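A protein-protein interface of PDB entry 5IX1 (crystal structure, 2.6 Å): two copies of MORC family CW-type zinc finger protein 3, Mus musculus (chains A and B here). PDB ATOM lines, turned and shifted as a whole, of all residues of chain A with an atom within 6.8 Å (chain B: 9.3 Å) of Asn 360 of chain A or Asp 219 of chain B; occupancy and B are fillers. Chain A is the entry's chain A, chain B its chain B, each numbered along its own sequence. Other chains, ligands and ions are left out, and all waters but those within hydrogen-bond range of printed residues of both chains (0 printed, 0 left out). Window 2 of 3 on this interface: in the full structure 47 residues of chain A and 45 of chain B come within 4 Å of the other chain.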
ATOM      1  N   LYS A 288     -10.895 -21.060 -41.085  1.00  0.00           N
ATOM      2  CA  LYS A 288     -10.498 -19.692 -41.330  1.00  0.00           C
ATOM      3  C   LYS A 288      -9.071 -19.515 -40.891  1.00  0.00           C
ATOM      4  O   LYS A 288      -8.304 -18.808 -41.512  1.00  0.00           O
ATOM      5  CB  LYS A 288     -11.384 -18.761 -40.513  1.00  0.00           C
ATOM      6  CG  LYS A 288     -11.101 -18.815 -39.016  1.00  0.00           C
ATOM      7  CD  LYS A 288     -12.328 -18.568 -38.151  1.00  0.00           C
ATOM      8  CE  LYS A 288     -11.933 -18.272 -36.707  1.00  0.00           C
ATOM      9  NZ  LYS A 288     -13.067 -17.728 -35.903  1.00  0.00           N
ATOM     10  N   PHE A 289      -8.730 -20.149 -39.787  1.00  0.00           N
ATOM     11  CA  PHE A 289      -7.419 -19.988 -39.195  1.00  0.00           C
ATOM     12  C   PHE A 289      -6.298 -20.699 -39.918  1.00  0.00           C
ATOM     13  O   PHE A 289      -5.153 -20.560 -39.551  1.00  0.00           O
ATOM     14  CB  PHE A 289      -7.420 -20.350 -37.720  1.00  0.00           C
ATOM     15  CG  PHE A 289      -7.955 -21.706 -37.422  1.00  0.00           C
ATOM     16  CD1 PHE A 289      -7.116 -22.784 -37.352  1.00  0.00           C
ATOM     17  CD2 PHE A 289      -9.283 -21.889 -37.180  1.00  0.00           C
ATOM     18  CE1 PHE A 289      -7.598 -24.029 -37.064  1.00  0.00           C
ATOM     19  CE2 PHE A 289      -9.773 -23.131 -36.891  1.00  0.00           C
ATOM     20  CZ  PHE A 289      -8.928 -24.203 -36.835  1.00  0.00           C
ATOM     21  N   ASP A 357      -4.418 -29.566 -26.538  1.00  0.00           N
ATOM     22  CA  ASP A 357      -4.751 -28.419 -25.718  1.00  0.00           C
ATOM     23  C   ASP A 357      -6.125 -27.921 -26.065  1.00  0.00           C
ATOM     24  O   ASP A 357      -6.463 -27.769 -27.209  1.00  0.00           O
ATOM     25  CB  ASP A 357      -3.771 -27.300 -25.985  1.00  0.00           C
ATOM     26  CG  ASP A 357      -3.714 -26.307 -24.879  1.00  0.00           C
ATOM     27  OD1 ASP A 357      -4.418 -26.459 -23.887  1.00  0.00           O
ATOM     28  OD2 ASP A 357      -2.948 -25.358 -25.000  1.00  0.00           O
ATOM     29  N   TYR A 358      -6.904 -27.617 -25.051  1.00  0.00           N
ATOM     30  CA  TYR A 358      -8.292 -27.294 -25.248  1.00  0.00           C
ATOM     31  C   TYR A 358      -8.419 -25.844 -25.631  1.00  0.00           C
ATOM     32  O   TYR A 358      -8.859 -25.029 -24.863  1.00  0.00           O
ATOM     33  CB  TYR A 358      -9.055 -27.572 -23.971  1.00  0.00           C
ATOM     34  CG  TYR A 358     -10.537 -27.585 -24.138  1.00  0.00           C
ATOM     35  CD1 TYR A 358     -11.105 -27.875 -25.341  1.00  0.00           C
ATOM     36  CD2 TYR A 358     -11.365 -27.323 -23.083  1.00  0.00           C
ATOM     37  CE1 TYR A 358     -12.464 -27.898 -25.495  1.00  0.00           C
ATOM     38  CE2 TYR A 358     -12.728 -27.345 -23.228  1.00  0.00           C
ATOM     39  CZ  TYR A 358     -13.266 -27.628 -24.441  1.00  0.00           C
ATOM     40  OH  TYR A 358     -14.617 -27.652 -24.592  1.00  0.00           O
ATOM     41  N   THR A 359      -7.980 -25.543 -26.836  1.00  0.00           N
ATOM     42  CA  THR A 359      -8.014 -24.213 -27.374  1.00  0.00           C
ATOM     43  C   THR A 359      -9.246 -23.949 -28.176  1.00  0.00           C
ATOM     44  O   THR A 359     -10.053 -24.816 -28.378  1.00  0.00           O
ATOM     45  CB  THR A 359      -6.822 -23.927 -28.265  1.00  0.00           C
ATOM     46  OG1 THR A 359      -6.818 -24.851 -29.345  1.00  0.00           O
ATOM     47  CG2 THR A 359      -5.569 -24.061 -27.487  1.00  0.00           C
ATOM     48  N   ASN A 360      -9.389 -22.715 -28.616  1.00  0.00           N
ATOM     49  CA  ASN A 360     -10.521 -22.321 -29.415  1.00  0.00           C
ATOM     50  C   ASN A 360     -10.519 -23.091 -30.702  1.00  0.00           C
ATOM     51  O   ASN A 360     -11.538 -23.560 -31.156  1.00  0.00           O
ATOM     52  CB  ASN A 360     -10.434 -20.824 -29.689  1.00  0.00           C
ATOM     53  CG  ASN A 360     -11.440 -20.350 -30.708  1.00  0.00           C
ATOM     54  OD1 ASN A 360     -12.637 -20.542 -30.551  1.00  0.00           O
ATOM     55  ND2 ASN A 360     -10.953 -19.703 -31.750  1.00  0.00           N
ATOM     56  N   GLU A 361      -9.341 -23.238 -31.276  1.00  0.00           N
ATOM     57  CA  GLU A 361      -9.167 -23.969 -32.506  1.00  0.00           C
ATOM     58  C   GLU A 361      -9.537 -25.423 -32.337  1.00  0.00           C
ATOM     59  O   GLU A 361     -10.101 -26.022 -33.231  1.00  0.00           O
ATOM     60  CB  GLU A 361      -7.742 -23.835 -32.990  1.00  0.00           C
ATOM     61  CG  GLU A 361      -7.390 -22.422 -33.366  1.00  0.00           C
ATOM     62  CD  GLU A 361      -6.020 -22.313 -33.954  1.00  0.00           C
ATOM     63  OE1 GLU A 361      -5.138 -23.043 -33.505  1.00  0.00           O
ATOM     64  OE2 GLU A 361      -5.815 -21.509 -34.863  1.00  0.00           O
ATOM     65  N   TYR A 362      -9.199 -25.997 -31.199  1.00  0.00           N
ATOM     66  CA  TYR A 362      -9.553 -27.366 -30.956  1.00  0.00           C
ATOM     67  C   TYR A 362     -11.045 -27.488 -30.926  1.00  0.00           C
ATOM     68  O   TYR A 362     -11.614 -28.410 -31.476  1.00  0.00           O
ATOM     69  CB  TYR A 362      -8.960 -27.869 -29.657  1.00  0.00           C
ATOM     70  CG  TYR A 362      -9.467 -29.220 -29.295  1.00  0.00           C
ATOM     71  CD1 TYR A 362      -8.889 -30.354 -29.795  1.00  0.00           C
ATOM     72  CD2 TYR A 362     -10.551 -29.358 -28.484  1.00  0.00           C
ATOM     73  CE1 TYR A 362      -9.371 -31.595 -29.475  1.00  0.00           C
ATOM     74  CE2 TYR A 362     -11.041 -30.594 -28.159  1.00  0.00           C
ATOM     75  CZ  TYR A 362     -10.442 -31.707 -28.657  1.00  0.00           C
ATOM     76  OH  TYR A 362     -10.940 -32.934 -28.322  1.00  0.00           O
ATOM     77  N   ARG A 363     -11.683 -26.539 -30.276  1.00  0.00           N
ATOM     78  CA  ARG A 363     -13.111 -26.575 -30.122  1.00  0.00           C
ATOM     79  C   ARG A 363     -13.777 -26.479 -31.464  1.00  0.00           C
ATOM     80  O   ARG A 363     -14.741 -27.153 -31.729  1.00  0.00           O
ATOM     81  CB  ARG A 363     -13.554 -25.429 -29.231  1.00  0.00           C
ATOM     82  CG  ARG A 363     -13.990 -25.861 -27.850  1.00  0.00           C
ATOM     83  CD  ARG A 363     -14.240 -24.680 -26.941  1.00  0.00           C
ATOM     84  NE  ARG A 363     -13.106 -24.434 -26.073  1.00  0.00           N
ATOM     85  CZ  ARG A 363     -12.361 -23.349 -26.128  1.00  0.00           C
ATOM     86  NH1 ARG A 363     -12.645 -22.405 -26.992  1.00  0.00           N
ATOM     87  NH2 ARG A 363     -11.345 -23.204 -25.314  1.00  0.00           N
ATOM     88  N   LEU A 364     -13.258 -25.626 -32.317  1.00  0.00           N
ATOM     89  CA  LEU A 364     -13.825 -25.462 -33.629  1.00  0.00           C
ATOM     90  C   LEU A 364     -13.712 -26.731 -34.428  1.00  0.00           C
ATOM     91  O   LEU A 364     -14.624 -27.124 -35.120  1.00  0.00           O
ATOM     92  CB  LEU A 364     -13.118 -24.339 -34.360  1.00  0.00           C
ATOM     93  CG  LEU A 364     -13.474 -22.927 -33.922  1.00  0.00           C
ATOM     94  CD1 LEU A 364     -12.775 -21.895 -34.774  1.00  0.00           C
ATOM     95  CD2 LEU A 364     -14.969 -22.720 -33.962  1.00  0.00           C
ATOM     96  N   THR A 365     -12.570 -27.377 -34.323  1.00  0.00           N
ATOM     97  CA  THR A 365     -12.328 -28.569 -35.079  1.00  0.00           C
ATOM     98  C   THR A 365     -13.301 -29.636 -34.682  1.00  0.00           C
ATOM     99  O   THR A 365     -13.823 -30.332 -35.515  1.00  0.00           O
ATOM    100  CB  THR A 365     -10.909 -29.062 -34.858  1.00  0.00           C
ATOM    101  OG1 THR A 365     -10.001 -28.088 -35.352  1.00  0.00           O
ATOM    102  CG2 THR A 365     -10.686 -30.314 -35.603  1.00  0.00           C
ATOM    103  N   THR B  22      -4.836 -27.583 -19.114  1.00  0.00           N
ATOM    104  CA  THR B  22      -5.587 -27.276 -20.296  1.00  0.00           C
ATOM    105  C   THR B  22      -6.669 -26.271 -19.988  1.00  0.00           C
ATOM    106  O   THR B  22      -7.210 -25.645 -20.864  1.00  0.00           O
ATOM    107  CB  THR B  22      -6.246 -28.532 -20.852  1.00  0.00           C
ATOM    108  OG1 THR B  22      -6.857 -29.259 -19.793  1.00  0.00           O
ATOM    109  CG2 THR B  22      -5.235 -29.383 -21.482  1.00  0.00           C
ATOM    110  N   TYR B 199      -4.626 -14.846 -27.465  1.00  0.00           N
ATOM    111  CA  TYR B 199      -5.203 -15.265 -28.717  1.00  0.00           C
ATOM    112  C   TYR B 199      -6.006 -14.110 -29.263  1.00  0.00           C
ATOM    113  O   TYR B 199      -6.613 -13.366 -28.513  1.00  0.00           O
ATOM    114  CB  TYR B 199      -6.048 -16.524 -28.557  1.00  0.00           C
ATOM    115  CG  TYR B 199      -7.495 -16.294 -28.201  1.00  0.00           C
ATOM    116  CD1 TYR B 199      -8.502 -16.983 -28.854  1.00  0.00           C
ATOM    117  CD2 TYR B 199      -7.851 -15.388 -27.216  1.00  0.00           C
ATOM    118  CE1 TYR B 199      -9.824 -16.786 -28.535  1.00  0.00           C
ATOM    119  CE2 TYR B 199      -9.174 -15.182 -26.891  1.00  0.00           C
ATOM    120  CZ  TYR B 199     -10.150 -15.887 -27.556  1.00  0.00           C
ATOM    121  OH  TYR B 199     -11.464 -15.693 -27.245  1.00  0.00           O
ATOM    122  N   LYS B 200      -5.996 -13.957 -30.574  1.00  0.00           N
ATOM    123  CA  LYS B 200      -6.699 -12.857 -31.186  1.00  0.00           C
ATOM    124  C   LYS B 200      -6.052 -11.582 -30.729  1.00  0.00           C
ATOM    125  O   LYS B 200      -6.694 -10.559 -30.652  1.00  0.00           O
ATOM    126  CB  LYS B 200      -8.158 -12.852 -30.745  1.00  0.00           C
ATOM    127  CG  LYS B 200      -8.921 -14.124 -31.076  1.00  0.00           C
ATOM    128  CD  LYS B 200     -10.426 -13.892 -31.069  1.00  0.00           C
ATOM    129  CE  LYS B 200     -11.074 -14.443 -32.329  1.00  0.00           C
ATOM    130  NZ  LYS B 200     -12.175 -15.395 -32.019  1.00  0.00           N
ATOM    131  N   GLU B 204      -6.040 -14.559 -23.130  1.00  0.00           N
ATOM    132  CA  GLU B 204      -6.983 -15.647 -23.108  1.00  0.00           C
ATOM    133  C   GLU B 204      -8.053 -15.353 -22.108  1.00  0.00           C
ATOM    134  O   GLU B 204      -9.161 -15.802 -22.240  1.00  0.00           O
ATOM    135  CB  GLU B 204      -6.296 -16.970 -22.821  1.00  0.00           C
ATOM    136  CG  GLU B 204      -6.006 -17.258 -21.369  1.00  0.00           C
ATOM    137  CD  GLU B 204      -5.359 -18.601 -21.185  1.00  0.00           C
ATOM    138  OE1 GLU B 204      -4.437 -18.707 -20.371  1.00  0.00           O
ATOM    139  OE2 GLU B 204      -5.769 -19.549 -21.864  1.00  0.00           O
ATOM    140  N   ILE B 216     -13.255 -16.582 -18.422  1.00  0.00           N
ATOM    141  CA  ILE B 216     -12.846 -17.117 -19.684  1.00  0.00           C
ATOM    142  C   ILE B 216     -13.895 -16.729 -20.678  1.00  0.00           C
ATOM    143  O   ILE B 216     -15.068 -16.941 -20.456  1.00  0.00           O
ATOM    144  CB  ILE B 216     -12.719 -18.633 -19.616  1.00  0.00           C
ATOM    145  CG1 ILE B 216     -11.581 -19.009 -18.697  1.00  0.00           C
ATOM    146  CG2 ILE B 216     -12.467 -19.206 -20.990  1.00  0.00           C
ATOM    147  CD1 ILE B 216     -11.786 -20.335 -18.030  1.00  0.00           C
ATOM    148  N   PRO B 217     -13.402 -16.095 -21.822  1.00  0.00           N
ATOM    149  CA  PRO B 217     -14.452 -15.625 -22.723  1.00  0.00           C
ATOM    150  C   PRO B 217     -15.204 -16.732 -23.410  1.00  0.00           C
ATOM    151  O   PRO B 217     -14.690 -17.806 -23.550  1.00  0.00           O
ATOM    152  CB  PRO B 217     -13.696 -14.806 -23.747  1.00  0.00           C
ATOM    153  CG  PRO B 217     -12.401 -15.460 -23.859  1.00  0.00           C
ATOM    154  CD  PRO B 217     -12.061 -15.648 -22.445  1.00  0.00           C
ATOM    155  N   GLU B 218     -16.445 -16.477 -23.782  1.00  0.00           N
ATOM    156  CA  GLU B 218     -17.193 -17.377 -24.632  1.00  0.00           C
ATOM    157  C   GLU B 218     -16.683 -17.247 -26.041  1.00  0.00           C
ATOM    158  O   GLU B 218     -16.196 -16.210 -26.427  1.00  0.00           O
ATOM    159  CB  GLU B 218     -18.686 -17.079 -24.577  1.00  0.00           C
ATOM    160  CG  GLU B 218     -19.488 -17.671 -25.726  1.00  0.00           C
ATOM    161  CD  GLU B 218     -20.086 -19.027 -25.412  1.00  0.00           C
ATOM    162  OE1 GLU B 218     -20.229 -19.363 -24.222  1.00  0.00           O
ATOM    163  OE2 GLU B 218     -20.416 -19.756 -26.366  1.00  0.00           O
ATOM    164  N   ASP B 219     -16.795 -18.310 -26.814  1.00  0.00           N
ATOM    165  CA  ASP B 219     -16.251 -18.313 -28.154  1.00  0.00           C
ATOM    166  C   ASP B 219     -17.195 -17.617 -29.109  1.00  0.00           C
ATOM    167  O   ASP B 219     -16.770 -17.119 -30.142  1.00  0.00           O
ATOM    168  CB  ASP B 219     -15.992 -19.745 -28.630  1.00  0.00           C
ATOM    169  CG  ASP B 219     -15.200 -20.574 -27.627  1.00  0.00           C
ATOM    170  OD1 ASP B 219     -14.250 -20.045 -27.027  1.00  0.00           O
ATOM    171  OD2 ASP B 219     -15.526 -21.761 -27.451  1.00  0.00           O
ATOM    172  N   TYR B 229     -18.711 -20.804 -22.487  1.00  0.00           N
ATOM    173  CA  TYR B 229     -17.556 -21.687 -22.412  1.00  0.00           C
ATOM    174  C   TYR B 229     -17.782 -22.822 -21.439  1.00  0.00           C
ATOM    175  O   TYR B 229     -17.996 -22.601 -20.265  1.00  0.00           O
ATOM    176  CB  TYR B 229     -16.310 -20.917 -21.996  1.00  0.00           C
ATOM    177  CG  TYR B 229     -15.133 -21.793 -21.658  1.00  0.00           C
ATOM    178  CD1 TYR B 229     -14.169 -22.067 -22.589  1.00  0.00           C
ATOM    179  CD2 TYR B 229     -15.009 -22.359 -20.418  1.00  0.00           C
ATOM    180  CE1 TYR B 229     -13.103 -22.869 -22.290  1.00  0.00           C
ATOM    181  CE2 TYR B 229     -13.946 -23.165 -20.114  1.00  0.00           C
ATOM    182  CZ  TYR B 229     -12.999 -23.414 -21.059  1.00  0.00           C
ATOM    183  OH  TYR B 229     -11.931 -24.214 -20.776  1.00  0.00           O
ATOM    184  N   LYS B 230     -17.685 -24.043 -21.940  1.00  0.00           N
ATOM    185  CA  LYS B 230     -17.807 -25.224 -21.111  1.00  0.00           C
ATOM    186  C   LYS B 230     -16.462 -25.892 -21.069  1.00  0.00           C
ATOM    187  O   LYS B 230     -15.667 -25.740 -21.963  1.00  0.00           O
ATOM    188  CB  LYS B 230     -18.828 -26.207 -21.677  1.00  0.00           C
ATOM    189  CG  LYS B 230     -20.064 -25.583 -22.278  1.00  0.00           C
ATOM    190  CD  LYS B 230     -19.962 -25.470 -23.783  1.00  0.00           C
ATOM    191  CE  LYS B 230     -21.144 -24.704 -24.341  1.00  0.00           C
ATOM    192  NZ  LYS B 230     -20.831 -24.082 -25.655  1.00  0.00           N
ATOM    193  N   LYS B 231     -16.219 -26.633 -20.012  1.00  0.00           N
ATOM    194  CA  LYS B 231     -15.026 -27.430 -19.912  1.00  0.00           C
ATOM    195  C   LYS B 231     -15.140 -28.592 -20.870  1.00  0.00           C
ATOM    196  O   LYS B 231     -16.206 -28.877 -21.378  1.00  0.00           O
ATOM    197  CB  LYS B 231     -14.834 -27.929 -18.496  1.00  0.00           C
ATOM    198  CG  LYS B 231     -13.836 -27.106 -17.721  1.00  0.00           C
ATOM    199  CD  LYS B 231     -13.498 -27.753 -16.403  1.00  0.00           C
ATOM    200  CE  LYS B 231     -12.078 -28.248 -16.409  1.00  0.00           C
ATOM    201  NZ  LYS B 231     -11.678 -28.774 -15.087  1.00  0.00           N
ATOM    202  N   TYR B 244     -16.239 -20.985 -16.082  1.00  0.00           N
ATOM    203  CA  TYR B 244     -15.812 -19.734 -16.682  1.00  0.00           C
ATOM    204  C   TYR B 244     -15.522 -18.586 -15.736  1.00  0.00           C
ATOM    205  O   TYR B 244     -14.995 -17.585 -16.151  1.00  0.00           O
ATOM    206  CB  TYR B 244     -16.759 -19.311 -17.786  1.00  0.00           C
ATOM    207  CG  TYR B 244     -18.192 -19.238 -17.375  1.00  0.00           C
ATOM    208  CD1 TYR B 244     -18.658 -18.188 -16.623  1.00  0.00           C
ATOM    209  CD2 TYR B 244     -19.081 -20.201 -17.754  1.00  0.00           C
ATOM    210  CE1 TYR B 244     -19.970 -18.114 -16.246  1.00  0.00           C
ATOM    211  CE2 TYR B 244     -20.393 -20.134 -17.382  1.00  0.00           C
ATOM    212  CZ  TYR B 244     -20.827 -19.083 -16.626  1.00  0.00           C
ATOM    213  OH  TYR B 244     -22.128 -18.999 -16.248  1.00  0.00           O
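The backbone carbonyl oxygen of Lys 230 of chain B is in hydrogen-bond range of the side-chain hydroxyl of Tyr 358 of chain A, at 3.4 Å. The guanidinium group (NH1) of Arg 363 of chain A lies within salt-bridge range of the side-chain carboxylate (OD1) of Asp 219 of chain B (2.9 Å).
Among the printed residues, merely in contact across the chains: Asp 357 of chain A with Thr 22 of chain B (3.9 Å), Tyr 358 of chain A with Tyr 229 of chain B (3.9 Å), Tyr 358 of chain A with Lys 231 of chain B (3.6 Å), Asn 360 of chain A with Asp 219 of chain B (3.9 Å) and Arg 363 of chain A with Tyr 229 of chain B (3.5 Å).
O of Tyr 358 of chain A is in hydrogen-bond range of NH2 of Arg 363 of chain A, at 3.1 Å. The side-chain carboxylate of Glu 218 of chain B lies within hydrogen-bond range of the backbone NH of Tyr 229 of chain B, at 2.7 Å.
No position is printed for both chains. Of the 7 pairs that touch across the chains among the printed residues, none has its exchanged pair printed and touching as well.
Asp 219 of chain B touches just these residues of chain A: Asn 360 and Arg 363. Printed residues of chain B within 4 Å of Asp 357 of chain A: Thr 22. Of the printed residues of chain A, Thr 22 of chain B touches Asp 357. Printed residues of chain A within 4 Å of Lys 230 of chain B: Tyr 358. The nearest residue of chain B that does not touch Asn 360 of chain A is Tyr 199 of chain B (4.2 Å). The nearest residue of chain A that does not touch Asp 219 of chain B is Leu 364 of chain A (6.2 Å). The nearest printed residue of chain A that does not touch Lys 231 of chain B is Arg 363 of chain A (7.0 Å).
Of the 12 printed residues of chain B, 5 touch a printed residue of chain A. Printed residues of chain B that touch a printed residue of chain A: Thr 22, Asp 219, Tyr 229, Lys 230 and Lys 231. Hydrophobic or aromatic side chains of chain B that line the printed part of chain A: Tyr 229. Among the printed residues, Asp or Glu carboxylates within 4 Å of a Lys or Arg side-chain nitrogen of the other chain: Arg 363 of chain A with Asp 219 of chain B (2.9 Å).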
